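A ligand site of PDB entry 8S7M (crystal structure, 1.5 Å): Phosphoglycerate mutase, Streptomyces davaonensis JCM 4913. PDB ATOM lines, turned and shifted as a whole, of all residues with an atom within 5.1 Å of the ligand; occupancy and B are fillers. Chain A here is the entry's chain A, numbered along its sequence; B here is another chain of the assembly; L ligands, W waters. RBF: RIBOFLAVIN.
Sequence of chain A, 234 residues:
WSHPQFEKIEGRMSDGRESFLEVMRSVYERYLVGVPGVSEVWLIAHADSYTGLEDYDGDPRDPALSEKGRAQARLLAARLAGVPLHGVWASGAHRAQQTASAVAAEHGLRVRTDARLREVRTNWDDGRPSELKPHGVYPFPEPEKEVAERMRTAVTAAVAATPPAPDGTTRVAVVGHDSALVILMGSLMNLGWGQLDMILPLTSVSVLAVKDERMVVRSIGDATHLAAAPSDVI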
ATOM      1  N   HIS A  46     -14.056 -31.944 -39.890  1.00  0.00           N
ATOM      2  CA  HIS A  46     -15.091 -32.718 -40.572  1.00  0.00           C
ATOM      3  C   HIS A  46     -16.478 -32.072 -40.391  1.00  0.00           C
ATOM      4  O   HIS A  46     -16.697 -31.203 -39.541  1.00  0.00           O
ATOM      5  CB  HIS A  46     -15.152 -34.150 -40.030  1.00  0.00           C
ATOM      6  CG  HIS A  46     -15.536 -34.229 -38.598  1.00  0.00           C
ATOM      7  ND1 HIS A  46     -16.846 -34.112 -38.169  1.00  0.00           N
ATOM      8  CD2 HIS A  46     -14.786 -34.426 -37.475  1.00  0.00           C
ATOM      9  CE1 HIS A  46     -16.885 -34.217 -36.849  1.00  0.00           C
ATOM     10  NE2 HIS A  46     -15.657 -34.403 -36.409  1.00  0.00           N
ATOM     11  N   TYR A  50     -23.392 -34.959 -35.529  1.00  0.00           N
ATOM     12  CA  TYR A  50     -24.033 -34.922 -34.229  1.00  0.00           C
ATOM     13  C   TYR A  50     -25.536 -34.655 -34.256  1.00  0.00           C
ATOM     14  O   TYR A  50     -26.238 -35.051 -33.327  1.00  0.00           O
ATOM     15  CB  TYR A  50     -23.325 -33.903 -33.333  1.00  0.00           C
ATOM     16  CG  TYR A  50     -21.830 -34.118 -33.379  1.00  0.00           C
ATOM     17  CD1 TYR A  50     -21.284 -35.291 -32.863  1.00  0.00           C
ATOM     18  CD2 TYR A  50     -20.981 -33.207 -33.979  1.00  0.00           C
ATOM     19  CE1 TYR A  50     -19.931 -35.534 -32.908  1.00  0.00           C
ATOM     20  CE2 TYR A  50     -19.612 -33.436 -34.032  1.00  0.00           C
ATOM     21  CZ  TYR A  50     -19.095 -34.613 -33.492  1.00  0.00           C
ATOM     22  OH  TYR A  50     -17.749 -34.868 -33.523  1.00  0.00           O
ATOM     23  N   GLU A 119      -9.041 -37.812 -33.704  1.00  0.00           N
ATOM     24  CA  GLU A 119      -9.372 -36.869 -32.648  1.00  0.00           C
ATOM     25  C   GLU A 119      -8.668 -37.252 -31.339  1.00  0.00           C
ATOM     26  O   GLU A 119      -8.298 -38.403 -31.112  1.00  0.00           O
ATOM     27  CB  GLU A 119     -10.894 -36.820 -32.432  1.00  0.00           C
ATOM     28  CG  GLU A 119     -11.436 -35.736 -31.421  1.00  0.00           C
ATOM     29  CD  GLU A 119     -10.981 -34.289 -31.684  1.00  0.00           C
ATOM     30  OE1 GLU A 119      -9.789 -34.006 -31.595  1.00  0.00           O
ATOM     31  OE2 GLU A 119     -11.852 -33.432 -31.947  1.00  0.00           O
ATOM     32  N   SER A 130     -18.882 -37.574 -20.115  1.00  0.00           N
ATOM     33  CA  SER A 130     -18.288 -36.308 -20.508  1.00  0.00           C
ATOM     34  C   SER A 130     -18.516 -35.282 -19.410  1.00  0.00           C
ATOM     35  O   SER A 130     -19.565 -35.261 -18.769  1.00  0.00           O
ATOM     36  CB  SER A 130     -18.903 -35.830 -21.829  1.00  0.00           C
ATOM     37  OG  SER A 130     -18.704 -36.796 -22.860  1.00  0.00           O
ATOM     38  N   GLU A 131     -17.518 -34.441 -19.162  1.00  0.00           N
ATOM     39  CA  GLU A 131     -17.580 -33.482 -18.078  1.00  0.00           C
ATOM     40  C   GLU A 131     -17.268 -32.126 -18.669  1.00  0.00           C
ATOM     41  O   GLU A 131     -16.319 -31.989 -19.453  1.00  0.00           O
ATOM     42  CB  GLU A 131     -16.559 -33.870 -17.008  1.00  0.00           C
ATOM     43  CG  GLU A 131     -16.269 -32.834 -15.944  1.00  0.00           C
ATOM     44  CD  GLU A 131     -15.204 -33.323 -14.969  1.00  0.00           C
ATOM     45  OE1 GLU A 131     -14.552 -32.478 -14.311  1.00  0.00           O
ATOM     46  OE2 GLU A 131     -14.958 -34.553 -14.919  1.00  0.00           O
ATOM     47  N   LEU A 132     -18.081 -31.136 -18.340  1.00  0.00           N
ATOM     48  CA  LEU A 132     -17.852 -29.770 -18.809  1.00  0.00           C
ATOM     49  C   LEU A 132     -16.822 -29.128 -17.888  1.00  0.00           C
ATOM     50  O   LEU A 132     -17.113 -28.846 -16.719  1.00  0.00           O
ATOM     51  CB  LEU A 132     -19.162 -28.996 -18.774  1.00  0.00           C
ATOM     52  CG  LEU A 132     -19.085 -27.498 -19.064  1.00  0.00           C
ATOM     53  CD1 LEU A 132     -18.849 -27.234 -20.555  1.00  0.00           C
ATOM     54  CD2 LEU A 132     -20.344 -26.795 -18.578  1.00  0.00           C
ATOM     55  N   LYS A 133     -15.591 -28.873 -18.433  1.00  0.00           N
ATOM     56  CA  LYS A 133     -14.549 -28.213 -17.662  1.00  0.00           C
ATOM     57  C   LYS A 133     -14.701 -26.700 -17.757  1.00  0.00           C
ATOM     58  O   LYS A 133     -15.187 -26.177 -18.771  1.00  0.00           O
ATOM     59  CB  LYS A 133     -13.182 -28.580 -18.225  1.00  0.00           C
ATOM     60  CG  LYS A 133     -12.814 -30.044 -18.101  1.00  0.00           C
ATOM     61  CD  LYS A 133     -12.829 -30.552 -16.665  1.00  0.00           C
ATOM     62  CE  LYS A 133     -12.649 -32.061 -16.595  1.00  0.00           C
ATOM     63  NZ  LYS A 133     -11.342 -32.552 -17.112  1.00  0.00           N
ATOM     64  N   PRO A 139      -9.643 -30.849 -21.050  1.00  0.00           N
ATOM     65  CA  PRO A 139     -10.731 -31.788 -20.758  1.00  0.00           C
ATOM     66  C   PRO A 139     -10.547 -33.205 -21.278  1.00  0.00           C
ATOM     67  O   PRO A 139     -11.494 -33.991 -21.179  1.00  0.00           O
ATOM     68  CB  PRO A 139     -11.914 -31.139 -21.483  1.00  0.00           C
ATOM     69  CG  PRO A 139     -11.275 -30.587 -22.738  1.00  0.00           C
ATOM     70  CD  PRO A 139      -9.911 -30.076 -22.286  1.00  0.00           C
ATOM     71  N   PHE A 140      -9.372 -33.565 -21.792  1.00  0.00           N
ATOM     72  CA  PHE A 140      -9.245 -34.876 -22.435  1.00  0.00           C
ATOM     73  C   PHE A 140      -8.220 -35.758 -21.725  1.00  0.00           C
ATOM     74  O   PHE A 140      -7.281 -35.272 -21.104  1.00  0.00           O
ATOM     75  CB  PHE A 140      -8.787 -34.705 -23.890  1.00  0.00           C
ATOM     76  CG  PHE A 140      -9.625 -33.733 -24.665  1.00  0.00           C
ATOM     77  CD1 PHE A 140     -10.932 -34.038 -24.978  1.00  0.00           C
ATOM     78  CD2 PHE A 140      -9.094 -32.533 -25.092  1.00  0.00           C
ATOM     79  CE1 PHE A 140     -11.704 -33.149 -25.705  1.00  0.00           C
ATOM     80  CE2 PHE A 140      -9.854 -31.637 -25.821  1.00  0.00           C
ATOM     81  CZ  PHE A 140     -11.150 -31.934 -26.135  1.00  0.00           C
ATOM     82  N   ASP A 178     -11.846 -31.213 -34.703  1.00  0.00           N
ATOM     83  CA  ASP A 178     -11.659 -29.820 -34.297  1.00  0.00           C
ATOM     84  C   ASP A 178     -10.762 -29.655 -33.063  1.00  0.00           C
ATOM     85  O   ASP A 178      -9.990 -28.690 -32.996  1.00  0.00           O
ATOM     86  CB  ASP A 178     -12.994 -29.089 -34.213  1.00  0.00           C
ATOM     87  CG  ASP A 178     -13.896 -29.618 -33.134  1.00  0.00           C
ATOM     88  OD1 ASP A 178     -13.675 -29.330 -31.934  1.00  0.00           O
ATOM     89  OD2 ASP A 178     -14.870 -30.308 -33.509  1.00  0.00           O
ATOM     90  N   SER A 179     -10.834 -30.553 -32.086  1.00  0.00           N
ATOM     91  CA  SER A 179     -10.000 -30.361 -30.891  1.00  0.00           C
ATOM     92  C   SER A 179      -8.526 -30.606 -31.189  1.00  0.00           C
ATOM     93  O   SER A 179      -7.654 -29.806 -30.815  1.00  0.00           O
ATOM     94  CB  SER A 179     -10.515 -31.211 -29.733  1.00  0.00           C
ATOM     95  OG  SER A 179     -11.739 -30.671 -29.244  1.00  0.00           O
ATOM     96  N   VAL A 182      -7.178 -27.562 -33.173  1.00  0.00           N
ATOM     97  CA  VAL A 182      -6.893 -26.321 -32.461  1.00  0.00           C
ATOM     98  C   VAL A 182      -5.717 -26.535 -31.500  1.00  0.00           C
ATOM     99  O   VAL A 182      -4.943 -25.603 -31.246  1.00  0.00           O
ATOM    100  CB  VAL A 182      -8.181 -25.804 -31.796  1.00  0.00           C
ATOM    101  CG1 VAL A 182      -8.436 -26.535 -30.511  1.00  0.00           C
ATOM    102  CG2 VAL A 182      -8.123 -24.290 -31.608  1.00  0.00           C
ATOM    103  N   TRP A 193      -3.270 -25.103 -24.053  1.00  0.00           N
ATOM    104  CA  TRP A 193      -4.722 -25.224 -24.137  1.00  0.00           C
ATOM    105  C   TRP A 193      -5.384 -24.071 -23.399  1.00  0.00           C
ATOM    106  O   TRP A 193      -5.015 -23.738 -22.267  1.00  0.00           O
ATOM    107  CB  TRP A 193      -5.182 -26.541 -23.532  1.00  0.00           C
ATOM    108  CG  TRP A 193      -6.689 -26.699 -23.562  1.00  0.00           C
ATOM    109  CD1 TRP A 193      -7.563 -26.413 -22.554  1.00  0.00           C
ATOM    110  CD2 TRP A 193      -7.475 -27.186 -24.649  1.00  0.00           C
ATOM    111  NE1 TRP A 193      -8.854 -26.669 -22.957  1.00  0.00           N
ATOM    112  CE2 TRP A 193      -8.820 -27.139 -24.242  1.00  0.00           C
ATOM    113  CE3 TRP A 193      -7.173 -27.629 -25.925  1.00  0.00           C
ATOM    114  CZ2 TRP A 193      -9.857 -27.552 -25.079  1.00  0.00           C
ATOM    115  CZ3 TRP A 193      -8.210 -28.042 -26.762  1.00  0.00           C
ATOM    116  CH2 TRP A 193      -9.538 -27.990 -26.327  1.00  0.00           C
ATOM    117  N   ASP A 197      -8.187 -19.326 -27.618  1.00  0.00           N
ATOM    118  CA  ASP A 197      -9.457 -19.710 -27.021  1.00  0.00           C
ATOM    119  C   ASP A 197     -10.553 -19.698 -28.089  1.00  0.00           C
ATOM    120  O   ASP A 197     -11.349 -18.766 -28.190  1.00  0.00           O
ATOM    121  CB  ASP A 197      -9.810 -18.792 -25.855  1.00  0.00           C
ATOM    122  CG  ASP A 197     -11.041 -19.251 -25.117  1.00  0.00           C
ATOM    123  OD1 ASP A 197     -11.353 -20.467 -25.177  1.00  0.00           O
ATOM    124  OD2 ASP A 197     -11.718 -18.409 -24.518  1.00  0.00           O
ATOM    125  N   MET A 198     -10.617 -20.793 -28.842  1.00  0.00           N
ATOM    126  CA  MET A 198     -11.543 -20.889 -29.958  1.00  0.00           C
ATOM    127  C   MET A 198     -11.999 -22.333 -30.094  1.00  0.00           C
ATOM    128  O   MET A 198     -11.240 -23.260 -29.794  1.00  0.00           O
ATOM    129  CB  MET A 198     -10.839 -20.560 -31.275  1.00  0.00           C
ATOM    130  CG  MET A 198     -10.454 -19.104 -31.381  1.00  0.00           C
ATOM    131  SD  MET A 198      -9.415 -18.856 -32.836  1.00  0.00           S
ATOM    132  CE  MET A 198     -10.667 -18.869 -34.137  1.00  0.00           C
ATOM    133  N   ILE A 199     -13.229 -22.512 -30.570  1.00  0.00           N
ATOM    134  CA  ILE A 199     -13.664 -23.801 -31.102  1.00  0.00           C
ATOM    135  C   ILE A 199     -13.807 -23.657 -32.613  1.00  0.00           C
ATOM    136  O   ILE A 199     -14.277 -22.627 -33.099  1.00  0.00           O
ATOM    137  CB  ILE A 199     -14.947 -24.338 -30.431  1.00  0.00           C
ATOM    138  CG1 ILE A 199     -15.193 -25.787 -30.862  1.00  0.00           C
ATOM    139  CG2 ILE A 199     -16.150 -23.428 -30.680  1.00  0.00           C
ATOM    140  CD1 ILE A 199     -16.117 -26.582 -29.942  1.00  0.00           C
ATOM    141  N   LEU A 202     -17.583 -26.918 -37.612  1.00  0.00           N
ATOM    142  CA  LEU A 202     -17.546 -28.071 -38.521  1.00  0.00           C
ATOM    143  C   LEU A 202     -17.493 -27.585 -39.971  1.00  0.00           C
ATOM    144  O   LEU A 202     -18.170 -26.631 -40.347  1.00  0.00           O
ATOM    145  CB  LEU A 202     -18.776 -28.936 -38.269  1.00  0.00           C
ATOM    146  CG  LEU A 202     -18.878 -29.406 -36.803  1.00  0.00           C
ATOM    147  CD1 LEU A 202     -20.051 -30.339 -36.623  1.00  0.00           C
ATOM    148  CD2 LEU A 202     -17.610 -30.094 -36.325  1.00  0.00           C
ATOM    149  N   PHE B  20     -22.153 -36.778 -24.002  1.00  0.00           N
ATOM    150  CA  PHE B  20     -21.277 -36.148 -24.992  1.00  0.00           C
ATOM    151  C   PHE B  20     -21.970 -34.974 -25.670  1.00  0.00           C
ATOM    152  O   PHE B  20     -21.411 -33.875 -25.769  1.00  0.00           O
ATOM    153  CB  PHE B  20     -20.855 -37.203 -26.012  1.00  0.00           C
ATOM    154  CG  PHE B  20     -20.021 -36.640 -27.126  1.00  0.00           C
ATOM    155  CD1 PHE B  20     -18.674 -36.382 -26.935  1.00  0.00           C
ATOM    156  CD2 PHE B  20     -20.601 -36.330 -28.347  1.00  0.00           C
ATOM    157  CE1 PHE B  20     -17.898 -35.844 -27.972  1.00  0.00           C
ATOM    158  CE2 PHE B  20     -19.842 -35.791 -29.379  1.00  0.00           C
ATOM    159  CZ  PHE B  20     -18.494 -35.548 -29.185  1.00  0.00           C
ATOM    160  N   VAL B  23     -22.705 -31.897 -23.207  1.00  0.00           N
ATOM    161  CA  VAL B  23     -21.498 -31.138 -22.907  1.00  0.00           C
ATOM    162  C   VAL B  23     -21.056 -30.344 -24.124  1.00  0.00           C
ATOM    163  O   VAL B  23     -20.696 -29.168 -24.016  1.00  0.00           O
ATOM    164  CB  VAL B  23     -20.402 -32.077 -22.382  1.00  0.00           C
ATOM    165  CG1 VAL B  23     -19.046 -31.368 -22.404  1.00  0.00           C
ATOM    166  CG2 VAL B  23     -20.758 -32.587 -20.999  1.00  0.00           C
ATOM    167  N   MET B  24     -21.087 -30.974 -25.309  1.00  0.00           N
ATOM    168  CA  MET B  24     -20.757 -30.242 -26.525  1.00  0.00           C
ATOM    169  C   MET B  24     -21.659 -29.030 -26.679  1.00  0.00           C
ATOM    170  O   MET B  24     -21.193 -27.949 -27.072  1.00  0.00           O
ATOM    171  CB  MET B  24     -20.922 -31.136 -27.757  1.00  0.00           C
ATOM    172  CG  MET B  24     -20.825 -30.359 -29.070  1.00  0.00           C
ATOM    173  SD  MET B  24     -20.599 -31.475 -30.434  1.00  0.00           S
ATOM    174  CE  MET B  24     -22.175 -32.308 -30.364  1.00  0.00           C
ATOM    175  N   VAL B  27     -20.418 -26.338 -24.416  1.00  0.00           N
ATOM    176  CA  VAL B  27     -19.201 -25.720 -24.936  1.00  0.00           C
ATOM    177  C   VAL B  27     -19.535 -24.768 -26.079  1.00  0.00           C
ATOM    178  O   VAL B  27     -19.051 -23.635 -26.131  1.00  0.00           O
ATOM    179  CB  VAL B  27     -18.178 -26.796 -25.359  1.00  0.00           C
ATOM    180  CG1 VAL B  27     -16.999 -26.160 -26.097  1.00  0.00           C
ATOM    181  CG2 VAL B  27     -17.682 -27.563 -24.139  1.00  0.00           C
ATOM    182  N   ARG B  30     -20.797 -21.361 -24.906  1.00  0.00           N
ATOM    183  CA  ARG B  30     -19.775 -20.440 -24.403  1.00  0.00           C
ATOM    184  C   ARG B  30     -19.202 -19.594 -25.520  1.00  0.00           C
ATOM    185  O   ARG B  30     -18.726 -18.483 -25.280  1.00  0.00           O
ATOM    186  CB  ARG B  30     -18.622 -21.206 -23.768  1.00  0.00           C
ATOM    187  CG  ARG B  30     -18.881 -21.814 -22.434  1.00  0.00           C
ATOM    188  CD  ARG B  30     -17.599 -22.429 -21.956  1.00  0.00           C
ATOM    189  NE  ARG B  30     -17.749 -23.130 -20.690  1.00  0.00           N
ATOM    190  CZ  ARG B  30     -16.858 -23.977 -20.207  1.00  0.00           C
ATOM    191  NH1 ARG B  30     -15.743 -24.240 -20.854  1.00  0.00           N
ATOM    192  NH2 ARG B  30     -17.109 -24.593 -19.048  1.00  0.00           N
ATOM    193  N   TYR B  31     -19.184 -20.131 -26.728  1.00  0.00           N
ATOM    194  CA  TYR B  31     -18.655 -19.422 -27.873  1.00  0.00           C
ATOM    195  C   TYR B  31     -19.782 -18.835 -28.723  1.00  0.00           C
ATOM    196  O   TYR B  31     -19.580 -18.549 -29.913  1.00  0.00           O
ATOM    197  CB  TYR B  31     -17.705 -20.331 -28.646  1.00  0.00           C
ATOM    198  CG  TYR B  31     -16.556 -20.746 -27.761  1.00  0.00           C
ATOM    199  CD1 TYR B  31     -15.421 -19.952 -27.653  1.00  0.00           C
ATOM    200  CD2 TYR B  31     -16.635 -21.888 -26.988  1.00  0.00           C
ATOM    201  CE1 TYR B  31     -14.389 -20.307 -26.806  1.00  0.00           C
ATOM    202  CE2 TYR B  31     -15.608 -22.249 -26.134  1.00  0.00           C
ATOM    203  CZ  TYR B  31     -14.485 -21.454 -26.062  1.00  0.00           C
ATOM    204  OH  TYR B  31     -13.459 -21.804 -25.227  1.00  0.00           O
HETATM  205  N1  RBF L   1     -15.272 -31.642 -24.382  1.00  0.00           N
HETATM  206  C2  RBF L   1     -15.629 -32.094 -23.120  1.00  0.00           C
HETATM  207  O2  RBF L   1     -16.153 -33.236 -23.026  1.00  0.00           O
HETATM  208  N3  RBF L   1     -15.516 -31.318 -22.020  1.00  0.00           N
HETATM  209  C4  RBF L   1     -15.151 -29.997 -22.155  1.00  0.00           C
HETATM  210  O4  RBF L   1     -15.055 -29.249 -21.131  1.00  0.00           O
HETATM  211  C4A RBF L   1     -14.670 -29.512 -23.465  1.00  0.00           C
HETATM  212  N5  RBF L   1     -14.257 -28.194 -23.635  1.00  0.00           N
HETATM  213  C5A RBF L   1     -13.886 -27.776 -24.891  1.00  0.00           C
HETATM  214  C6  RBF L   1     -13.282 -26.519 -25.043  1.00  0.00           C
HETATM  215  C7  RBF L   1     -12.872 -26.089 -26.325  1.00  0.00           C
HETATM  216  C7M RBF L   1     -12.374 -24.638 -26.490  1.00  0.00           C
HETATM  217  C8  RBF L   1     -12.927 -26.986 -27.429  1.00  0.00           C
HETATM  218  C8M RBF L   1     -12.181 -26.810 -28.772  1.00  0.00           C
HETATM  219  C9  RBF L   1     -13.426 -28.277 -27.209  1.00  0.00           C
HETATM  220  C9A RBF L   1     -13.895 -28.668 -25.938  1.00  0.00           C
HETATM  221  N10 RBF L   1     -14.439 -29.922 -25.824  1.00  0.00           N
HETATM  222  C10 RBF L   1     -14.846 -30.348 -24.566  1.00  0.00           C
HETATM  223  C1' RBF L   1     -14.737 -30.721 -26.970  1.00  0.00           C
HETATM  224  C2' RBF L   1     -16.142 -30.321 -27.502  1.00  0.00           C
HETATM  225  O2' RBF L   1     -17.083 -30.315 -26.474  1.00  0.00           O
HETATM  226  C3' RBF L   1     -16.650 -31.332 -28.573  1.00  0.00           C
HETATM  227  O3' RBF L   1     -16.620 -32.627 -28.092  1.00  0.00           O
HETATM  228  C4' RBF L   1     -15.812 -31.260 -29.830  1.00  0.00           C
HETATM  229  O4' RBF L   1     -15.558 -29.932 -30.146  1.00  0.00           O
HETATM  230  C5' RBF L   1     -16.669 -31.933 -30.930  1.00  0.00           C
HETATM  231  O5' RBF L   1     -15.840 -32.111 -32.097  1.00  0.00           O
HETATM  232  O   HOH W   1     -10.069 -23.002 -24.754  1.00  0.00           O
HETATM  233  O   HOH W   2     -14.163 -26.141 -21.536  1.00  0.00           O
HETATM  234  O   HOH W   3     -15.343 -34.864 -21.052  1.00  0.00           O
HETATM  235  O   HOH W   4     -18.399 -32.971 -25.794  1.00  0.00           O
HETATM  236  O   HOH W   5     -14.893 -34.920 -24.789  1.00  0.00           O
HETATM  237  O   HOH W   6     -12.076 -26.810 -31.968  1.00  0.00           O
HETATM  238  O   HOH W   7     -14.340 -33.985 -31.810  1.00  0.00           O
HETATM  239  O   HOH W   8     -14.890 -34.281 -27.548  1.00  0.00           O
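OD2 of Asp 178 sits at hydrogen-bond distance from O5' of the ligand. O of Glu 131 sits at hydrogen-bond distance from N3 of the ligand, at 2.8 Å. N of Lys 133 lies within hydrogen-bond range of O4 of the ligand (2.8 Å).
OH of Tyr 31 of chain B is in hydrogen-bond range of OD1 of Asp 197 (2.5 Å). The backbone NH (N) of Ser 179 lies within hydrogen-bond range of the side-chain carboxylate (OE2) of Glu 119 (3.1 Å). O of Lys 133 sits at hydrogen-bond distance from NH2 of Arg 30 of chain B (2.5 Å).
Residues that only touch the ligand: Tyr 50, Ser 130, Leu 132, Pro 139, Phe 140, Ser 179, Trp 193, Met 198, Ile 199, Phe 20 of chain B, Val 23 of chain B, Met 24 of chain B, Val 27 of chain B and Tyr 31 of chain B. 17 residues have an atom within 4 Å of the ligand: Tyr 50, Ser 130, Glu 131, Leu 132, Lys 133, Pro 139, Phe 140, Asp 178, Ser 179, Trp 193, Met 198, Ile 199, Phe 20 of chain B, Val 23 of chain B, Met 24 of chain B, Val 27 of chain B and Tyr 31 of chain B. Along chain A the residues within 4 Å of the ligand span positions 50 to 199.
Water W7 lies within hydrogen-bond range of O5' of the ligand (2.4 Å) and OE2 of Glu 119 (2.6 Å). Water W3 lies within hydrogen-bond range of O2 of the ligand (2.7 Å) and N of Glu 131 (2.9 Å). Water W4 lies within hydrogen-bond range of O3' of the ligand (2.9 Å), O of Phe 20 of chain B (3.1 Å) and N of Met 24 of chain B (3.4 Å). Water W2 lies within hydrogen-bond range of NH1 of Arg 30 of chain B (2.6 Å), N5 of the ligand (2.9 Å) and O of Lys 133 (2.9 Å).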
